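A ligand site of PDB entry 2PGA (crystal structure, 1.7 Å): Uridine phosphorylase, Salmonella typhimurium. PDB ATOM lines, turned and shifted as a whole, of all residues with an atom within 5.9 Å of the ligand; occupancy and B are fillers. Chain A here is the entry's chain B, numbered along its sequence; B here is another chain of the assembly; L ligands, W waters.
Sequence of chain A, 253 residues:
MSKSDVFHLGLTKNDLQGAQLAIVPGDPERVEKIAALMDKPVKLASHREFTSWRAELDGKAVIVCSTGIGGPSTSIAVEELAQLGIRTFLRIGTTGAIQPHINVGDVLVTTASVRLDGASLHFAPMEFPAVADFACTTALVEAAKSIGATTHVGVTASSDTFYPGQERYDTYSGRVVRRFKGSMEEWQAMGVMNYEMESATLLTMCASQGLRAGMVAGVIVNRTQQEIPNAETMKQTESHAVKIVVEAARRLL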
ATOM      1  N   GLY A  26     -25.414   3.067  22.955  1.00  0.00           N
ATOM      2  CA  GLY A  26     -24.943   3.854  24.074  1.00  0.00           C
ATOM      3  C   GLY A  26     -25.520   5.252  24.064  1.00  0.00           C
ATOM      4  O   GLY A  26     -25.847   5.809  25.104  1.00  0.00           O
ATOM      5  N   GLY A  68     -26.466   4.822  27.856  1.00  0.00           N
ATOM      6  CA  GLY A  68     -25.511   5.828  28.294  1.00  0.00           C
ATOM      7  C   GLY A  68     -24.105   5.269  28.121  1.00  0.00           C
ATOM      8  O   GLY A  68     -23.922   4.112  27.771  1.00  0.00           O
ATOM      9  N   ILE A  69     -23.091   6.084  28.387  1.00  0.00           N
ATOM     10  CA  ILE A  69     -21.722   5.594  28.337  1.00  0.00           C
ATOM     11  C   ILE A  69     -21.335   4.868  29.617  1.00  0.00           C
ATOM     12  O   ILE A  69     -21.508   5.389  30.700  1.00  0.00           O
ATOM     13  CB  ILE A  69     -20.736   6.758  28.148  1.00  0.00           C
ATOM     14  CG1 ILE A  69     -20.870   7.362  26.756  1.00  0.00           C
ATOM     15  CG2 ILE A  69     -19.310   6.284  28.361  1.00  0.00           C
ATOM     16  CD1 ILE A  69     -20.012   8.568  26.560  1.00  0.00           C
ATOM     17  N   GLY A  70     -20.789   3.664  29.494  1.00  0.00           N
ATOM     18  CA  GLY A  70     -20.166   3.029  30.632  1.00  0.00           C
ATOM     19  C   GLY A  70     -20.971   1.911  31.257  1.00  0.00           C
ATOM     20  O   GLY A  70     -22.201   1.839  31.131  1.00  0.00           O
ATOM     21  N   ARG A  91     -25.998  -5.097  21.937  1.00  0.00           N
ATOM     22  CA  ARG A  91     -25.390  -3.785  22.004  1.00  0.00           C
ATOM     23  C   ARG A  91     -24.866  -3.405  20.620  1.00  0.00           C
ATOM     24  O   ARG A  91     -24.237  -4.205  19.936  1.00  0.00           O
ATOM     25  CB  ARG A  91     -24.257  -3.716  23.034  1.00  0.00           C
ATOM     26  CG  ARG A  91     -23.505  -2.385  22.985  1.00  0.00           C
ATOM     27  CD  ARG A  91     -22.616  -2.136  24.207  1.00  0.00           C
ATOM     28  NE  ARG A  91     -21.380  -1.487  23.765  1.00  0.00           N
ATOM     29  CZ  ARG A  91     -21.301  -0.232  23.333  1.00  0.00           C
ATOM     30  NH1 ARG A  91     -22.387   0.529  23.314  1.00  0.00           N
ATOM     31  NH2 ARG A  91     -20.135   0.263  22.920  1.00  0.00           N
ATOM     32  N   GLY A  93     -22.572  -0.358  19.152  1.00  0.00           N
ATOM     33  CA  GLY A  93     -21.763   0.735  19.655  1.00  0.00           C
ATOM     34  C   GLY A  93     -20.870   1.362  18.625  1.00  0.00           C
ATOM     35  O   GLY A  93     -20.946   1.043  17.426  1.00  0.00           O
ATOM     36  N   THR A  94     -20.039   2.279  19.087  1.00  0.00           N
ATOM     37  CA  THR A  94     -18.933   2.803  18.307  1.00  0.00           C
ATOM     38  C   THR A  94     -17.639   2.436  19.014  1.00  0.00           C
ATOM     39  O   THR A  94     -17.630   2.175  20.224  1.00  0.00           O
ATOM     40  CB  THR A  94     -19.016   4.342  18.114  1.00  0.00           C
ATOM     41  OG1 THR A  94     -19.039   4.988  19.398  1.00  0.00           O
ATOM     42  CG2 THR A  94     -20.260   4.726  17.322  1.00  0.00           C
ATOM     43  N   THR A  95     -16.543   2.418  18.275  1.00  0.00           N
ATOM     44  CA  THR A  95     -15.330   1.839  18.822  1.00  0.00           C
ATOM     45  C   THR A  95     -14.063   2.392  18.187  1.00  0.00           C
ATOM     46  O   THR A  95     -14.074   2.837  17.031  1.00  0.00           O
ATOM     47  CB  THR A  95     -15.374   0.301  18.650  1.00  0.00           C
ATOM     48  OG1 THR A  95     -14.287  -0.296  19.370  1.00  0.00           O
ATOM     49  CG2 THR A  95     -15.304  -0.091  17.183  1.00  0.00           C
ATOM     50  N   GLY A  96     -12.977   2.379  18.945  1.00  0.00           N
ATOM     51  CA  GLY A  96     -11.669   2.690  18.411  1.00  0.00           C
ATOM     52  C   GLY A  96     -10.909   1.402  18.109  1.00  0.00           C
ATOM     53  O   GLY A  96     -10.712   0.581  19.006  1.00  0.00           O
ATOM     54  N   PHE A 162     -12.593   6.591  28.978  1.00  0.00           N
ATOM     55  CA  PHE A 162     -12.300   6.893  27.591  1.00  0.00           C
ATOM     56  C   PHE A 162     -10.820   7.223  27.458  1.00  0.00           C
ATOM     57  O   PHE A 162     -10.189   6.913  26.443  1.00  0.00           O
ATOM     58  CB  PHE A 162     -13.150   8.098  27.139  1.00  0.00           C
ATOM     59  CG  PHE A 162     -13.016   8.432  25.680  1.00  0.00           C
ATOM     60  CD1 PHE A 162     -12.126   9.404  25.259  1.00  0.00           C
ATOM     61  CD2 PHE A 162     -13.797   7.787  24.733  1.00  0.00           C
ATOM     62  CE1 PHE A 162     -12.009   9.722  23.910  1.00  0.00           C
ATOM     63  CE2 PHE A 162     -13.694   8.103  23.383  1.00  0.00           C
ATOM     64  CZ  PHE A 162     -12.796   9.073  22.969  1.00  0.00           C
ATOM     65  N   GLN A 166      -7.775   3.634  28.080  1.00  0.00           N
ATOM     66  CA  GLN A 166      -7.530   3.296  26.672  1.00  0.00           C
ATOM     67  C   GLN A 166      -6.192   3.883  26.242  1.00  0.00           C
ATOM     68  O   GLN A 166      -5.934   4.079  25.059  1.00  0.00           O
ATOM     69  CB  GLN A 166      -8.669   3.813  25.784  1.00  0.00           C
ATOM     70  CG  GLN A 166     -10.055   3.335  26.255  1.00  0.00           C
ATOM     71  CD  GLN A 166     -11.158   3.656  25.269  1.00  0.00           C
ATOM     72  OE1 GLN A 166     -10.914   3.767  24.064  1.00  0.00           O
ATOM     73  NE2 GLN A 166     -12.389   3.786  25.767  1.00  0.00           N
ATOM     74  N   ARG A 168      -4.956   6.855  26.281  1.00  0.00           N
ATOM     75  CA  ARG A 168      -4.882   8.164  25.622  1.00  0.00           C
ATOM     76  C   ARG A 168      -4.054   9.130  26.464  1.00  0.00           C
ATOM     77  O   ARG A 168      -4.277   9.254  27.670  1.00  0.00           O
ATOM     78  CB  ARG A 168      -6.292   8.722  25.378  1.00  0.00           C
ATOM     79  CG  ARG A 168      -7.069   8.007  24.265  1.00  0.00           C
ATOM     80  CD  ARG A 168      -8.448   8.636  24.050  1.00  0.00           C
ATOM     81  NE  ARG A 168      -9.016   8.241  22.755  1.00  0.00           N
ATOM     82  CZ  ARG A 168      -9.958   7.315  22.565  1.00  0.00           C
ATOM     83  NH1 ARG A 168     -10.489   6.663  23.608  1.00  0.00           N
ATOM     84  NH2 ARG A 168     -10.363   7.047  21.326  1.00  0.00           N
ATOM     85  N   TYR A 195     -11.266  -0.980  21.360  1.00  0.00           N
ATOM     86  CA  TYR A 195     -11.658  -0.495  22.670  1.00  0.00           C
ATOM     87  C   TYR A 195     -13.093  -0.009  22.618  1.00  0.00           C
ATOM     88  O   TYR A 195     -13.485   0.660  21.658  1.00  0.00           O
ATOM     89  CB  TYR A 195     -10.853   0.751  23.037  1.00  0.00           C
ATOM     90  CG  TYR A 195      -9.482   0.566  23.639  1.00  0.00           C
ATOM     91  CD1 TYR A 195      -9.297  -0.127  24.833  1.00  0.00           C
ATOM     92  CD2 TYR A 195      -8.381   1.161  23.042  1.00  0.00           C
ATOM     93  CE1 TYR A 195      -8.042  -0.244  25.394  1.00  0.00           C
ATOM     94  CE2 TYR A 195      -7.114   1.054  23.608  1.00  0.00           C
ATOM     95  CZ  TYR A 195      -6.961   0.343  24.784  1.00  0.00           C
ATOM     96  OH  TYR A 195      -5.713   0.221  25.350  1.00  0.00           O
ATOM     97  N   GLU A 196     -13.860  -0.298  23.652  1.00  0.00           N
ATOM     98  CA  GLU A 196     -15.053   0.505  23.939  1.00  0.00           C
ATOM     99  C   GLU A 196     -15.272   0.478  25.444  1.00  0.00           C
ATOM    100  O   GLU A 196     -14.337   0.198  26.196  1.00  0.00           O
ATOM    101  CB  GLU A 196     -16.269   0.106  23.069  1.00  0.00           C
ATOM    102  CG  GLU A 196     -16.584  -1.387  23.028  1.00  0.00           C
ATOM    103  CD  GLU A 196     -17.176  -1.864  24.318  1.00  0.00           C
ATOM    104  OE1 GLU A 196     -18.395  -1.642  24.537  1.00  0.00           O
ATOM    105  OE2 GLU A 196     -16.424  -2.452  25.132  1.00  0.00           O
ATOM    106  N   MET A 197     -16.481   0.789  25.916  1.00  0.00           N
ATOM    107  CA  MET A 197     -16.632   1.023  27.360  1.00  0.00           C
ATOM    108  C   MET A 197     -17.804   0.312  28.021  1.00  0.00           C
ATOM    109  O   MET A 197     -18.051   0.505  29.207  1.00  0.00           O
ATOM    110  CB  MET A 197     -16.731   2.533  27.624  1.00  0.00           C
ATOM    111  CG  MET A 197     -15.479   3.298  27.215  1.00  0.00           C
ATOM    112  SD  MET A 197     -15.640   5.082  27.417  1.00  0.00           S
ATOM    113  CE  MET A 197     -15.912   5.175  29.183  1.00  0.00           C
ATOM    114  N   GLU A 198     -18.521  -0.523  27.284  1.00  0.00           N
ATOM    115  CA  GLU A 198     -19.734  -1.120  27.836  1.00  0.00           C
ATOM    116  C   GLU A 198     -19.793  -2.644  27.784  1.00  0.00           C
ATOM    117  O   GLU A 198     -20.534  -3.255  28.561  1.00  0.00           O
ATOM    118  CB  GLU A 198     -20.977  -0.538  27.149  1.00  0.00           C
ATOM    119  CG  GLU A 198     -21.175   0.965  27.397  1.00  0.00           C
ATOM    120  CD  GLU A 198     -20.232   1.847  26.600  1.00  0.00           C
ATOM    121  OE1 GLU A 198     -19.624   1.356  25.612  1.00  0.00           O
ATOM    122  OE2 GLU A 198     -20.090   3.030  26.965  1.00  0.00           O
ATOM    123  N   ILE A 220     -14.798   4.109  14.605  1.00  0.00           N
ATOM    124  CA  ILE A 220     -14.853   5.547  14.319  1.00  0.00           C
ATOM    125  C   ILE A 220     -13.467   6.187  14.387  1.00  0.00           C
ATOM    126  O   ILE A 220     -13.273   7.337  14.015  1.00  0.00           O
ATOM    127  CB  ILE A 220     -15.780   6.289  15.296  1.00  0.00           C
ATOM    128  CG1 ILE A 220     -15.298   6.097  16.735  1.00  0.00           C
ATOM    129  CG2 ILE A 220     -17.200   5.798  15.124  1.00  0.00           C
ATOM    130  CD1 ILE A 220     -15.696   7.226  17.665  1.00  0.00           C
ATOM    131  N   VAL A 221     -12.504   5.432  14.909  1.00  0.00           N
ATOM    132  CA  VAL A 221     -11.129   5.917  14.969  1.00  0.00           C
ATOM    133  C   VAL A 221     -10.177   4.731  15.003  1.00  0.00           C
ATOM    134  O   VAL A 221     -10.509   3.680  15.551  1.00  0.00           O
ATOM    135  CB  VAL A 221     -10.881   6.822  16.196  1.00  0.00           C
ATOM    136  CG1 VAL A 221     -10.985   6.021  17.506  1.00  0.00           C
ATOM    137  CG2 VAL A 221      -9.523   7.509  16.094  1.00  0.00           C
ATOM    138  N   ARG A 223      -6.670   3.742  16.492  1.00  0.00           N
ATOM    139  CA  ARG A 223      -5.762   4.240  17.529  1.00  0.00           C
ATOM    140  C   ARG A 223      -4.283   4.030  17.218  1.00  0.00           C
ATOM    141  O   ARG A 223      -3.423   4.567  17.912  1.00  0.00           O
ATOM    142  CB  ARG A 223      -6.108   3.601  18.876  1.00  0.00           C
ATOM    143  CG  ARG A 223      -7.478   3.996  19.430  1.00  0.00           C
ATOM    144  CD  ARG A 223      -7.469   5.444  19.927  1.00  0.00           C
ATOM    145  NE  ARG A 223      -6.285   5.704  20.741  1.00  0.00           N
ATOM    146  CZ  ARG A 223      -6.166   5.317  22.005  1.00  0.00           C
ATOM    147  NH1 ARG A 223      -7.173   4.679  22.585  1.00  0.00           N
ATOM    148  NH2 ARG A 223      -5.058   5.553  22.688  1.00  0.00           N
ATOM    149  N   GLU A 227      -5.638   9.503  18.510  1.00  0.00           N
ATOM    150  CA  GLU A 227      -6.438   9.244  19.709  1.00  0.00           C
ATOM    151  C   GLU A 227      -7.910   9.546  19.521  1.00  0.00           C
ATOM    152  O   GLU A 227      -8.756   8.883  20.109  1.00  0.00           O
ATOM    153  CB  GLU A 227      -5.869  10.024  20.902  1.00  0.00           C
ATOM    154  CG  GLU A 227      -4.479   9.558  21.276  1.00  0.00           C
ATOM    155  CD  GLU A 227      -4.034  10.084  22.614  1.00  0.00           C
ATOM    156  OE1 GLU A 227      -4.756  10.913  23.212  1.00  0.00           O
ATOM    157  OE2 GLU A 227      -2.954   9.647  23.076  1.00  0.00           O
ATOM    158  N   PHE B   7     -14.065  16.178  22.668  1.00  0.00           N
ATOM    159  CA  PHE B   7     -14.750  15.149  21.886  1.00  0.00           C
ATOM    160  C   PHE B   7     -16.216  14.891  22.244  1.00  0.00           C
ATOM    161  O   PHE B   7     -17.041  14.651  21.354  1.00  0.00           O
ATOM    162  CB  PHE B   7     -13.966  13.846  21.921  1.00  0.00           C
ATOM    163  CG  PHE B   7     -14.486  12.821  20.962  1.00  0.00           C
ATOM    164  CD1 PHE B   7     -14.518  13.090  19.589  1.00  0.00           C
ATOM    165  CD2 PHE B   7     -14.943  11.590  21.415  1.00  0.00           C
ATOM    166  CE1 PHE B   7     -14.989  12.145  18.705  1.00  0.00           C
ATOM    167  CE2 PHE B   7     -15.415  10.645  20.531  1.00  0.00           C
ATOM    168  CZ  PHE B   7     -15.441  10.919  19.170  1.00  0.00           C
ATOM    169  N   HIS B   8     -16.552  14.938  23.533  1.00  0.00           N
ATOM    170  CA  HIS B   8     -17.905  14.584  23.957  1.00  0.00           C
ATOM    171  C   HIS B   8     -18.795  15.778  24.272  1.00  0.00           C
ATOM    172  O   HIS B   8     -19.955  15.799  23.863  1.00  0.00           O
ATOM    173  CB  HIS B   8     -17.867  13.636  25.161  1.00  0.00           C
ATOM    174  CG  HIS B   8     -17.225  12.325  24.861  1.00  0.00           C
ATOM    175  ND1 HIS B   8     -15.865  12.120  24.983  1.00  0.00           N
ATOM    176  CD2 HIS B   8     -17.737  11.148  24.420  1.00  0.00           C
ATOM    177  CE1 HIS B   8     -15.576  10.876  24.646  1.00  0.00           C
ATOM    178  NE2 HIS B   8     -16.690  10.266  24.301  1.00  0.00           N
ATOM    179  N   ARG B  48     -25.288  13.364  24.134  1.00  0.00           N
ATOM    180  CA  ARG B  48     -25.376  12.183  24.980  1.00  0.00           C
ATOM    181  C   ARG B  48     -25.928  12.579  26.343  1.00  0.00           C
ATOM    182  O   ARG B  48     -26.920  13.311  26.410  1.00  0.00           O
ATOM    183  CB  ARG B  48     -24.010  11.490  25.086  1.00  0.00           C
ATOM    184  CG  ARG B  48     -23.534  10.836  23.778  1.00  0.00           C
ATOM    185  CD  ARG B  48     -22.105  10.315  23.935  1.00  0.00           C
ATOM    186  NE  ARG B  48     -21.575   9.596  22.776  1.00  0.00           N
ATOM    187  CZ  ARG B  48     -21.660   8.271  22.602  1.00  0.00           C
ATOM    188  NH1 ARG B  48     -22.283   7.516  23.499  1.00  0.00           N
ATOM    189  NH2 ARG B  48     -21.122   7.708  21.520  1.00  0.00           N
ATOM    190  N   ILE B  76     -15.314  11.259  31.779  1.00  0.00           N
ATOM    191  CA  ILE B  76     -15.278  11.980  30.513  1.00  0.00           C
ATOM    192  C   ILE B  76     -15.620  13.455  30.727  1.00  0.00           C
ATOM    193  O   ILE B  76     -14.892  14.331  30.260  1.00  0.00           O
ATOM    194  CB  ILE B  76     -16.261  11.368  29.481  1.00  0.00           C
ATOM    195  CG1 ILE B  76     -15.733  10.016  28.991  1.00  0.00           C
ATOM    196  CG2 ILE B  76     -16.460  12.332  28.280  1.00  0.00           C
ATOM    197  CD1 ILE B  76     -16.718   9.247  28.083  1.00  0.00           C
HETATM  198  O1  LIG L   1     -19.792   4.494  24.902  1.00  0.00           O
HETATM  199  C1  LIG L   1     -18.461   4.903  24.626  1.00  0.00           C
HETATM  200  C2  LIG L   1     -17.718   3.861  23.826  1.00  0.00           C
HETATM  201  O2  LIG L   1     -16.350   4.025  24.235  1.00  0.00           O
HETATM  202  C3  LIG L   1     -15.623   4.025  23.021  1.00  0.00           C
HETATM  203  N1  LIG L   1     -14.205   4.333  22.920  1.00  0.00           N
HETATM  204  C4  LIG L   1     -13.749   4.893  21.795  1.00  0.00           C
HETATM  205  O3  LIG L   1     -12.512   5.074  21.688  1.00  0.00           O
HETATM  206  C5  LIG L   1     -14.621   5.307  20.771  1.00  0.00           C
HETATM  207  C6  LIG L   1     -16.009   5.123  20.876  1.00  0.00           C
HETATM  208  N2  LIG L   1     -16.481   4.539  21.978  1.00  0.00           N
HETATM  209  C7  LIG L   1     -17.846   4.272  22.341  1.00  0.00           C
HETATM  210  O4  LIG L   1     -18.491   5.545  22.371  1.00  0.00           O
HETATM  211  C8  LIG L   1     -18.457   6.093  23.689  1.00  0.00           C
HETATM  212  C9  LIG L   1     -17.182   6.899  23.916  1.00  0.00           C
HETATM  213  O5  LIG L   1     -17.118   8.013  23.035  1.00  0.00           O
HETATM  214  O   HOH W   1      -9.963   3.862  21.517  1.00  0.00           O
HETATM  215  O   HOH W   2     -18.485   8.792  20.730  1.00  0.00           O
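The side-chain carboxylate (OE2) of Glu 198 is in hydrogen-bond range of an oxygen (O1) of the ligand (2.5 Å). An oxygen (O5) of the ligand is in hydrogen-bond range of a ring nitrogen (NE2) of His 8 of chain B (2.6 Å). NH2 of Arg 168 lies within hydrogen-bond range of O3 of the ligand, 2.9 Å away. An oxygen (O4) of the ligand sits at hydrogen-bond distance from the side-chain hydroxyl (OG1) of Thr 94. The side-chain amide oxygen of Gln 166 lies close to an oxygen (O3) of the ligand, at 3.1 Å.
OE2 of Glu 198 is in hydrogen-bond range of N of Gly 70, 2.7 Å away. NH1 of Arg 168 lies within hydrogen-bond range of OE1 of Gln 166, 3.0 Å away. The guanidinium group (NH1) of Arg 168 is in hydrogen-bond range of the backbone carbonyl oxygen (O) of Phe 162 (2.9 Å). The side-chain sulfur of Met 197 sits close to the backbone NH of Phe 162 (3.7 Å). The side-chain carboxylate (OE1) of Glu 196 is in salt-bridge range of the guanidinium group (NH2) of Arg 91, 3.0 Å away. The backbone carbonyl oxygen of Thr 95 lies within hydrogen-bond range of the backbone NH of Ile 220 (2.8 Å). The side-chain hydroxyl of Thr 95 lies within hydrogen-bond range of the backbone carbonyl oxygen of Tyr 195, 2.6 Å away. N of Tyr 195 lies within hydrogen-bond range of O of Gly 96 (2.9 Å).
The side-chain sulfur (SD) of Met 197 sits close to an oxygen (O2) of the ligand (3.4 Å). Merely in contact with the ligand: Ile 69 (3.6 Å), Thr 95 (3.8 Å), Gly 96 (3.8 Å), Phe 162 (3.4 Å), Tyr 195 (3.9 Å), Glu 196 (3.7 Å), Ile 220 (3.8 Å) and Arg 48 of chain B (3.5 Å). Hydrophobic or aromatic side chains that line the ligand: Ile 69, Phe 162, Met 197, Ile 220 and His 8 of chain B. Within 4 Å of the ligand: Ile 69, Thr 94, Thr 95, Gly 96, Phe 162, Gln 166, Arg 168, Tyr 195, Glu 196, Met 197, Glu 198, Ile 220, His 8 of chain B and Arg 48 of chain B. The nearest printed residue that does not touch the ligand is Phe 7 of chain B (4.01 Å).
Water W2 lies within hydrogen-bond range of an oxygen (O5) of the ligand (2.8 Å) and the guanidinium group (NH2) of Arg 48 of chain B (3.0 Å). Water W1 lies within hydrogen-bond range of the side-chain amide oxygen (OE1) of Gln 166 (2.7 Å), an oxygen (O3) of the ligand (2.8 Å), the guanidinium group (NH1) of Arg 223 (3.1 Å) and the guanidinium group (NH2) of Arg 168 (3.2 Å).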
